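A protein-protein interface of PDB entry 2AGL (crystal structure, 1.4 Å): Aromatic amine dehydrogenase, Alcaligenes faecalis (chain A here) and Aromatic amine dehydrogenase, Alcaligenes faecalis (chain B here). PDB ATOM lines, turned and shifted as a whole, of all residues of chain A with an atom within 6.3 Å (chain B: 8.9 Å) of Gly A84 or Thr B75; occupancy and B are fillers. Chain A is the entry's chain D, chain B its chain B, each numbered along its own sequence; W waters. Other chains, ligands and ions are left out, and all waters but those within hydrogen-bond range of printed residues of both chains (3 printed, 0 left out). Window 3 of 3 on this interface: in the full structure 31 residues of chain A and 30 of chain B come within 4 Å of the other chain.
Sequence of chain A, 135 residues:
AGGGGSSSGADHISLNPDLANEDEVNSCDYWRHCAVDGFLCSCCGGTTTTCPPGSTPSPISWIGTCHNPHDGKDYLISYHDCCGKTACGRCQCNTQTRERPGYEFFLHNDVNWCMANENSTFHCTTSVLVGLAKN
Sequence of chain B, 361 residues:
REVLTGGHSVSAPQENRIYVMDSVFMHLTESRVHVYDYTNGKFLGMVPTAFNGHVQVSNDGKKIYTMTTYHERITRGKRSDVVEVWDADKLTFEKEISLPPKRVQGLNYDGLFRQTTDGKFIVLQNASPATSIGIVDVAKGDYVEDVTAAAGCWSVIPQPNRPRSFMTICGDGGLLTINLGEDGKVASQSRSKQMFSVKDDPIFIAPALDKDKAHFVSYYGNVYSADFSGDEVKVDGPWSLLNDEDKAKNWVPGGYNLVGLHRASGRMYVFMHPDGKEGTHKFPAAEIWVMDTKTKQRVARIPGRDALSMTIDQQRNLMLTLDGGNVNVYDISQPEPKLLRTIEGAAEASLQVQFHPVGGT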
ATOM      1  N   GLY A  54      36.136   3.087  18.016  1.00  0.00           N
ATOM      2  CA  GLY A  54      35.294   1.927  18.226  1.00  0.00           C
ATOM      3  C   GLY A  54      34.548   1.939  19.532  1.00  0.00           C
ATOM      4  O   GLY A  54      33.946   0.930  19.900  1.00  0.00           O
ATOM      5  N   SER A  55      34.616   3.020  20.304  1.00  0.00           N
ATOM      6  CA  SER A  55      33.796   3.178  21.486  1.00  0.00           C
ATOM      7  C   SER A  55      32.804   4.308  21.258  1.00  0.00           C
ATOM      8  O   SER A  55      33.092   5.269  20.528  1.00  0.00           O
ATOM      9  CB  SER A  55      34.628   3.422  22.756  1.00  0.00           C
ATOM     10  OG  SER A  55      35.364   4.629  22.687  1.00  0.00           O
ATOM     11  N   THR A  56      31.620   4.160  21.830  1.00  0.00           N
ATOM     12  CA  THR A  56      30.470   4.992  21.523  1.00  0.00           C
ATOM     13  C   THR A  56      30.187   5.968  22.667  1.00  0.00           C
ATOM     14  O   THR A  56      30.080   5.538  23.806  1.00  0.00           O
ATOM     15  CB  THR A  56      29.244   4.046  21.343  1.00  0.00           C
ATOM     16  OG1 THR A  56      29.538   3.063  20.329  1.00  0.00           O
ATOM     17  CG2 THR A  56      28.033   4.802  20.847  1.00  0.00           C
ATOM     18  N   CYS A  82      32.491   6.714  27.270  1.00  0.00           N
ATOM     19  CA  CYS A  82      32.637   6.017  26.014  1.00  0.00           C
ATOM     20  C   CYS A  82      32.403   4.552  26.333  1.00  0.00           C
ATOM     21  O   CYS A  82      32.900   4.022  27.350  1.00  0.00           O
ATOM     22  CB  CYS A  82      34.017   6.241  25.435  1.00  0.00           C
ATOM     23  SG  CYS A  82      34.272   7.970  25.032  1.00  0.00           S
ATOM     24  N   CYS A  83      31.638   3.907  25.461  1.00  0.00           N
ATOM     25  CA  CYS A  83      30.951   2.651  25.779  1.00  0.00           C
ATOM     26  C   CYS A  83      31.108   1.597  24.687  1.00  0.00           C
ATOM     27  O   CYS A  83      31.431   1.891  23.543  1.00  0.00           O
ATOM     28  CB  CYS A  83      29.461   2.954  25.974  1.00  0.00           C
ATOM     29  SG  CYS A  83      29.148   4.366  27.062  1.00  0.00           S
ATOM     30  N   GLY A  84      30.805   0.341  25.039  1.00  0.00           N
ATOM     31  CA  GLY A  84      30.772  -0.719  24.037  1.00  0.00           C
ATOM     32  C   GLY A  84      32.119  -1.361  23.756  1.00  0.00           C
ATOM     33  O   GLY A  84      32.281  -2.067  22.764  1.00  0.00           O
ATOM     34  N   LYS A  85      33.103  -1.101  24.622  1.00  0.00           N
ATOM     35  CA  LYS A  85      34.378  -1.813  24.674  1.00  0.00           C
ATOM     36  C   LYS A  85      34.709  -2.013  26.136  1.00  0.00           C
ATOM     37  O   LYS A  85      34.300  -1.247  27.016  1.00  0.00           O
ATOM     38  CB  LYS A  85      35.493  -1.012  23.984  1.00  0.00           C
ATOM     39  CG  LYS A  85      35.508  -1.108  22.490  1.00  0.00           C
ATOM     40  CD  LYS A  85      36.788  -0.605  21.844  1.00  0.00           C
ATOM     41  CE  LYS A  85      36.798  -1.042  20.416  1.00  0.00           C
ATOM     42  NZ  LYS A  85      37.849  -0.408  19.641  1.00  0.00           N
ATOM     43  N   THR A  86      35.456  -3.070  26.392  1.00  0.00           N
ATOM     44  CA  THR A  86      35.836  -3.401  27.743  1.00  0.00           C
ATOM     45  C   THR A  86      36.812  -2.388  28.340  1.00  0.00           C
ATOM     46  O   THR A  86      37.397  -1.551  27.631  1.00  0.00           O
ATOM     47  CB  THR A  86      36.406  -4.830  27.791  1.00  0.00           C
ATOM     48  OG1 THR A  86      37.328  -5.020  26.694  1.00  0.00           O
ATOM     49  CG2 THR A  86      35.265  -5.848  27.663  1.00  0.00           C
ATOM     50  N   CYS A 114      27.242   4.797  30.931  1.00  0.00           N
ATOM     51  CA  CYS A 114      26.912   4.007  29.734  1.00  0.00           C
ATOM     52  C   CYS A 114      25.603   3.203  29.881  1.00  0.00           C
ATOM     53  O   CYS A 114      25.257   2.447  28.970  1.00  0.00           O
ATOM     54  CB  CYS A 114      28.032   2.993  29.445  1.00  0.00           C
ATOM     55  SG  CYS A 114      29.584   3.674  28.879  1.00  0.00           S
ATOM     56  N   ASN A 117      23.241   3.035  26.892  1.00  0.00           N
ATOM     57  CA  ASN A 117      23.780   2.800  25.540  1.00  0.00           C
ATOM     58  C   ASN A 117      23.357   1.433  25.011  1.00  0.00           C
ATOM     59  O   ASN A 117      23.018   0.530  25.769  1.00  0.00           O
ATOM     60  CB  ASN A 117      25.308   2.883  25.534  1.00  0.00           C
ATOM     61  CG  ASN A 117      25.814   4.272  25.293  1.00  0.00           C
ATOM     62  OD1 ASN A 117      26.562   4.519  24.320  1.00  0.00           O
ATOM     63  ND2 ASN A 117      25.455   5.188  26.160  1.00  0.00           N
ATOM     64  N   ASN A 119      25.238  -0.806  23.896  1.00  0.00           N
ATOM     65  CA  ASN A 119      26.057  -1.681  24.730  1.00  0.00           C
ATOM     66  C   ASN A 119      26.611  -0.910  25.909  1.00  0.00           C
ATOM     67  O   ASN A 119      27.351   0.069  25.723  1.00  0.00           O
ATOM     68  CB  ASN A 119      27.183  -2.313  23.985  1.00  0.00           C
ATOM     69  CG  ASN A 119      27.833  -3.384  24.822  1.00  0.00           C
ATOM     70  OD1 ASN A 119      28.820  -3.142  25.539  1.00  0.00           O
ATOM     71  ND2 ASN A 119      27.250  -4.569  24.798  1.00  0.00           N
ATOM     72  N   SER A 120      26.264  -1.359  27.112  1.00  0.00           N
ATOM     73  CA  SER A 120      26.577  -0.657  28.350  1.00  0.00           C
ATOM     74  C   SER A 120      27.964  -0.943  28.911  1.00  0.00           C
ATOM     75  O   SER A 120      28.291  -0.402  29.956  1.00  0.00           O
ATOM     76  CB  SER A 120      25.505  -0.947  29.397  1.00  0.00           C
ATOM     77  OG  SER A 120      25.358  -2.330  29.600  1.00  0.00           O
ATOM     78  N   THR A 121      28.786  -1.736  28.256  1.00  0.00           N
ATOM     79  CA  THR A 121      30.119  -1.993  28.798  1.00  0.00           C
ATOM     80  C   THR A 121      30.911  -0.687  28.844  1.00  0.00           C
ATOM     81  O   THR A 121      30.958   0.091  27.869  1.00  0.00           O
ATOM     82  CB  THR A 121      30.886  -2.994  27.938  1.00  0.00           C
ATOM     83  OG1 THR A 121      30.078  -4.158  27.707  1.00  0.00           O
ATOM     84  CG2 THR A 121      32.149  -3.487  28.635  1.00  0.00           C
ATOM     85  N   PHE A 122      31.520  -0.430  29.980  1.00  0.00           N
ATOM     86  CA  PHE A 122      32.210   0.828  30.223  1.00  0.00           C
ATOM     87  C   PHE A 122      33.653   0.785  29.760  1.00  0.00           C
ATOM     88  O   PHE A 122      34.424  -0.085  30.168  1.00  0.00           O
ATOM     89  CB  PHE A 122      32.165   1.193  31.694  1.00  0.00           C
ATOM     90  CG  PHE A 122      33.056   2.366  32.044  1.00  0.00           C
ATOM     91  CD1 PHE A 122      32.762   3.670  31.621  1.00  0.00           C
ATOM     92  CD2 PHE A 122      34.212   2.160  32.780  1.00  0.00           C
ATOM     93  CE1 PHE A 122      33.579   4.702  31.967  1.00  0.00           C
ATOM     94  CE2 PHE A 122      35.039   3.205  33.111  1.00  0.00           C
ATOM     95  CZ  PHE A 122      34.721   4.467  32.706  1.00  0.00           C
ATOM     96  N   HIS A 123      34.031   1.743  28.919  1.00  0.00           N
ATOM     97  CA  HIS A 123      35.373   1.830  28.375  1.00  0.00           C
ATOM     98  C   HIS A 123      36.237   2.919  29.040  1.00  0.00           C
ATOM     99  O   HIS A 123      37.343   2.621  29.551  1.00  0.00           O
ATOM    100  CB  HIS A 123      35.330   2.000  26.855  1.00  0.00           C
ATOM    101  CG  HIS A 123      36.676   1.977  26.206  1.00  0.00           C
ATOM    102  ND1 HIS A 123      37.556   0.927  26.366  1.00  0.00           N
ATOM    103  CD2 HIS A 123      37.308   2.873  25.408  1.00  0.00           C
ATOM    104  CE1 HIS A 123      38.671   1.186  25.713  1.00  0.00           C
ATOM    105  NE2 HIS A 123      38.546   2.361  25.110  1.00  0.00           N
ATOM    106  N   THR B  29      33.783  -6.965  33.245  1.00  0.00           N
ATOM    107  CA  THR B  29      32.976  -8.067  32.722  1.00  0.00           C
ATOM    108  C   THR B  29      33.217  -9.403  33.391  1.00  0.00           C
ATOM    109  O   THR B  29      32.473 -10.338  33.101  1.00  0.00           O
ATOM    110  CB  THR B  29      33.145  -8.255  31.190  1.00  0.00           C
ATOM    111  OG1 THR B  29      34.472  -8.651  30.865  1.00  0.00           O
ATOM    112  CG2 THR B  29      32.763  -6.976  30.391  1.00  0.00           C
ATOM    113  N   PHE B  51      29.201  -8.840  34.141  1.00  0.00           N
ATOM    114  CA  PHE B  51      29.491  -7.415  34.177  1.00  0.00           C
ATOM    115  C   PHE B  51      28.911  -6.769  35.422  1.00  0.00           C
ATOM    116  O   PHE B  51      27.699  -6.754  35.595  1.00  0.00           O
ATOM    117  CB  PHE B  51      28.934  -6.698  32.952  1.00  0.00           C
ATOM    118  CG  PHE B  51      29.194  -5.221  32.941  1.00  0.00           C
ATOM    119  CD1 PHE B  51      30.460  -4.731  32.652  1.00  0.00           C
ATOM    120  CD2 PHE B  51      28.171  -4.326  33.193  1.00  0.00           C
ATOM    121  CE1 PHE B  51      30.692  -3.386  32.625  1.00  0.00           C
ATOM    122  CE2 PHE B  51      28.420  -2.943  33.164  1.00  0.00           C
ATOM    123  CZ  PHE B  51      29.685  -2.492  32.894  1.00  0.00           C
ATOM    124  N   TYR B  70      24.274  -9.409  31.006  1.00  0.00           N
ATOM    125  CA  TYR B  70      24.894 -10.111  29.910  1.00  0.00           C
ATOM    126  C   TYR B  70      24.537  -9.435  28.582  1.00  0.00           C
ATOM    127  O   TYR B  70      23.519  -8.755  28.483  1.00  0.00           O
ATOM    128  CB  TYR B  70      24.383 -11.553  29.795  1.00  0.00           C
ATOM    129  CG  TYR B  70      24.647 -12.428  30.987  1.00  0.00           C
ATOM    130  CD1 TYR B  70      23.700 -12.570  31.991  1.00  0.00           C
ATOM    131  CD2 TYR B  70      25.836 -13.110  31.110  1.00  0.00           C
ATOM    132  CE1 TYR B  70      23.922 -13.367  33.074  1.00  0.00           C
ATOM    133  CE2 TYR B  70      26.063 -13.944  32.196  1.00  0.00           C
ATOM    134  CZ  TYR B  70      25.100 -14.033  33.189  1.00  0.00           C
ATOM    135  OH  TYR B  70      25.353 -14.902  34.265  1.00  0.00           O
ATOM    136  N   HIS B  71      25.388  -9.623  27.572  1.00  0.00           N
ATOM    137  CA  HIS B  71      25.007  -9.348  26.174  1.00  0.00           C
ATOM    138  C   HIS B  71      25.400 -10.549  25.326  1.00  0.00           C
ATOM    139  O   HIS B  71      26.360 -11.253  25.653  1.00  0.00           O
ATOM    140  CB  HIS B  71      25.677  -8.099  25.612  1.00  0.00           C
ATOM    141  CG  HIS B  71      25.316  -6.835  26.304  1.00  0.00           C
ATOM    142  ND1 HIS B  71      24.373  -5.944  25.835  1.00  0.00           N
ATOM    143  CD2 HIS B  71      25.813  -6.291  27.435  1.00  0.00           C
ATOM    144  CE1 HIS B  71      24.300  -4.910  26.655  1.00  0.00           C
ATOM    145  NE2 HIS B  71      25.168  -5.100  27.631  1.00  0.00           N
ATOM    146  N   GLU B  72      24.702 -10.747  24.200  1.00  0.00           N
ATOM    147  CA  GLU B  72      24.915 -11.953  23.412  1.00  0.00           C
ATOM    148  C   GLU B  72      26.381 -12.124  22.990  1.00  0.00           C
ATOM    149  O   GLU B  72      26.896 -13.239  22.925  1.00  0.00           O
ATOM    150  CB  GLU B  72      24.046 -11.971  22.162  1.00  0.00           C
ATOM    151  CG  GLU B  72      22.533 -11.886  22.329  1.00  0.00           C
ATOM    152  CD  GLU B  72      21.786 -11.698  20.988  1.00  0.00           C
ATOM    153  OE1 GLU B  72      21.979 -10.674  20.247  1.00  0.00           O
ATOM    154  OE2 GLU B  72      20.949 -12.576  20.668  1.00  0.00           O
ATOM    155  N   ARG B  73      27.073 -11.011  22.746  1.00  0.00           N
ATOM    156  CA  ARG B  73      28.473 -11.010  22.396  1.00  0.00           C
ATOM    157  C   ARG B  73      29.297 -10.032  23.279  1.00  0.00           C
ATOM    158  O   ARG B  73      30.301  -9.471  22.820  1.00  0.00           O
ATOM    159  CB  ARG B  73      28.618 -10.675  20.896  1.00  0.00           C
ATOM    160  CG  ARG B  73      28.097 -11.789  20.000  1.00  0.00           C
ATOM    161  CD  ARG B  73      28.999 -12.991  19.947  1.00  0.00           C
ATOM    162  NE  ARG B  73      28.548 -13.979  18.964  1.00  0.00           N
ATOM    163  CZ  ARG B  73      27.675 -14.927  19.185  1.00  0.00           C
ATOM    164  NH1 ARG B  73      27.127 -15.100  20.368  1.00  0.00           N
ATOM    165  NH2 ARG B  73      27.347 -15.717  18.176  1.00  0.00           N
ATOM    166  N   ILE B  74      28.852  -9.862  24.526  1.00  0.00           N
ATOM    167  CA  ILE B  74      29.517  -9.077  25.586  1.00  0.00           C
ATOM    168  C   ILE B  74      29.457  -7.559  25.325  1.00  0.00           C
ATOM    169  O   ILE B  74      28.778  -6.825  26.050  1.00  0.00           O
ATOM    170  CB  ILE B  74      30.939  -9.573  25.900  1.00  0.00           C
ATOM    171  CG1 ILE B  74      30.948 -11.084  26.133  1.00  0.00           C
ATOM    172  CG2 ILE B  74      31.465  -8.846  27.140  1.00  0.00           C
ATOM    173  CD1 ILE B  74      32.294 -11.690  26.175  1.00  0.00           C
ATOM    174  N   THR B  75      30.211  -7.107  24.313  1.00  0.00           N
ATOM    175  CA  THR B  75      30.295  -5.697  23.914  1.00  0.00           C
ATOM    176  C   THR B  75      29.387  -5.361  22.731  1.00  0.00           C
ATOM    177  O   THR B  75      29.341  -4.194  22.302  1.00  0.00           O
ATOM    178  CB  THR B  75      31.714  -5.388  23.563  1.00  0.00           C
ATOM    179  OG1 THR B  75      32.251  -6.411  22.708  1.00  0.00           O
ATOM    180  CG2 THR B  75      32.612  -5.422  24.807  1.00  0.00           C
ATOM    181  N   ARG B  76      28.614  -6.332  22.258  1.00  0.00           N
ATOM    182  CA  ARG B  76      27.568  -6.106  21.277  1.00  0.00           C
ATOM    183  C   ARG B  76      26.481  -7.174  21.478  1.00  0.00           C
ATOM    184  O   ARG B  76      26.665  -8.139  22.221  1.00  0.00           O
ATOM    185  CB  ARG B  76      28.124  -6.088  19.840  1.00  0.00           C
ATOM    186  CG  ARG B  76      28.730  -7.385  19.423  1.00  0.00           C
ATOM    187  CD  ARG B  76      29.425  -7.363  18.061  1.00  0.00           C
ATOM    188  NE  ARG B  76      30.142  -8.597  17.827  1.00  0.00           N
ATOM    189  CZ  ARG B  76      29.605  -9.687  17.299  1.00  0.00           C
ATOM    190  NH1 ARG B  76      28.347  -9.668  16.883  1.00  0.00           N
ATOM    191  NH2 ARG B  76      30.343 -10.784  17.202  1.00  0.00           N
ATOM    192  N   GLY B  77      25.348  -6.984  20.831  1.00  0.00           N
ATOM    193  CA  GLY B  77      24.241  -7.935  20.875  1.00  0.00           C
ATOM    194  C   GLY B  77      23.250  -7.588  21.977  1.00  0.00           C
ATOM    195  O   GLY B  77      23.416  -6.659  22.759  1.00  0.00           O
ATOM    196  N   LYS B  78      22.206  -8.402  22.053  1.00  0.00           N
ATOM    197  CA  LYS B  78      21.088  -8.122  22.921  1.00  0.00           C
ATOM    198  C   LYS B  78      21.497  -8.201  24.394  1.00  0.00           C
ATOM    199  O   LYS B  78      22.231  -9.091  24.775  1.00  0.00           O
ATOM    200  CB  LYS B  78      19.921  -9.069  22.636  1.00  0.00           C
ATOM    201  CG  LYS B  78      18.658  -8.684  23.406  1.00  0.00           C
ATOM    202  CD  LYS B  78      17.506  -9.621  23.115  1.00  0.00           C
ATOM    203  CE  LYS B  78      16.172  -9.080  23.647  1.00  0.00           C
ATOM    204  NZ  LYS B  78      15.027  -9.900  23.140  1.00  0.00           N
HETATM  205  O   HOH W   1      30.071  -2.124  20.583  1.00  0.00           O
HETATM  206  O   HOH W   2      23.474  -2.163  27.054  1.00  0.00           O
HETATM  207  O   HOH W   3      24.995  -4.426  22.907  1.00  0.00           O
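Printed residues of chain B that touch a printed residue of chain A: Thr B29, Phe B51, His B71, Ile B74, Thr B75 and Arg B76. Hydrophobic or aromatic side chains of chain B that line the printed part of chain A: Phe B51 and His B71.
Thr B75 touches Gly A84 (CB to O, 3.5 Å). Thr B29 touches Thr A86. Thr B75 touches Thr A86 (CG2 to CG2, 3.9 Å). Phe B51 touches Ser A120 (CZ to O, 3.9 Å). Thr A121 touches Thr B29.
ND2 of Asn A119 sits close to ND1 of His B71 (3.4 Å). ND2 of Asn A119 is in hydrogen-bond range of O of Ile B74 (3.0 Å). The side-chain amide nitrogen (ND2) of Asn A119 lies close to the backbone carbonyl oxygen (O) of Thr B75 (3.3 Å). The side-chain amide nitrogen (ND2) of Asn A119 lies close to the backbone NH (N) of Arg B76 (3.4 Å). NE2 of His B71 lies within hydrogen-bond range of OG of Ser A120. The side-chain hydroxyl (OG1) of Thr A121 lies within hydrogen-bond range of the backbone carbonyl oxygen (O) of Ile B74.
The backbone NH (N) of Gly A84 is in hydrogen-bond range of the backbone carbonyl oxygen (O) of Thr A121, 2.8 Å away. The backbone carbonyl oxygen of Thr A86 lies within hydrogen-bond range of a ring nitrogen (ND1) of His A123, at 2.8 Å. The side-chain amide oxygen of Asn A119 lies within hydrogen-bond range of the side-chain hydroxyl of Thr A121, 2.7 Å away. A ring nitrogen (ND1) of His B71 lies within hydrogen-bond range of the backbone carbonyl oxygen (O) of Gly B77, 3.3 Å away. SG of Cys A83 forms a disulfide with SG of Cys A114, 2.0 Å away.
Of the printed residues of chain B, Gly A84 touches Thr B75 (3.5 Å). Thr B75 touches three residues of chain A. Printed residues of chain B within 4 Å of Thr A86: Thr B29 and Thr B75. Of the printed residues of chain B, Asn A119 touches His B71 (3.3 Å), Ile B74 (3.0 Å), Thr B75 (3.0 Å) and Arg B76 (3.4 Å). Of the printed residues of chain B, Ser A120 touches Phe B51 and His B71. Of the printed residues of chain A, Ile B74 touches Asn A119 and Thr A121. Of the printed residues of chain A, Thr B29 touches Thr A86 and Thr A121. Phe A122 touches none of the printed residues of chain B. Thr A56 touches none of the printed residues of chain B. The nearest residue of chain B that does not touch Gly A84 is Arg B76 (5.6 Å). The nearest printed residue of chain A that does not touch His B71 is Thr A121 (4.8 Å).
Water W3 lies within hydrogen-bond range of the backbone carbonyl oxygen (O) of Gly B77 (2.7 Å), the side-chain amide nitrogen (ND2) of Asn A119 (2.9 Å) and a ring nitrogen (ND1) of His B71 (3.4 Å). Water W1 lies within hydrogen-bond range of O of Thr B75 (2.8 Å) and O of Gly A84 (3.1 Å). Water W2 lies within hydrogen-bond range of the backbone NH of Ser A120 (2.9 Å), the backbone carbonyl oxygen of Asn A117 (3.0 Å) and a ring nitrogen (NE2) of His B71 (3.4 Å).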
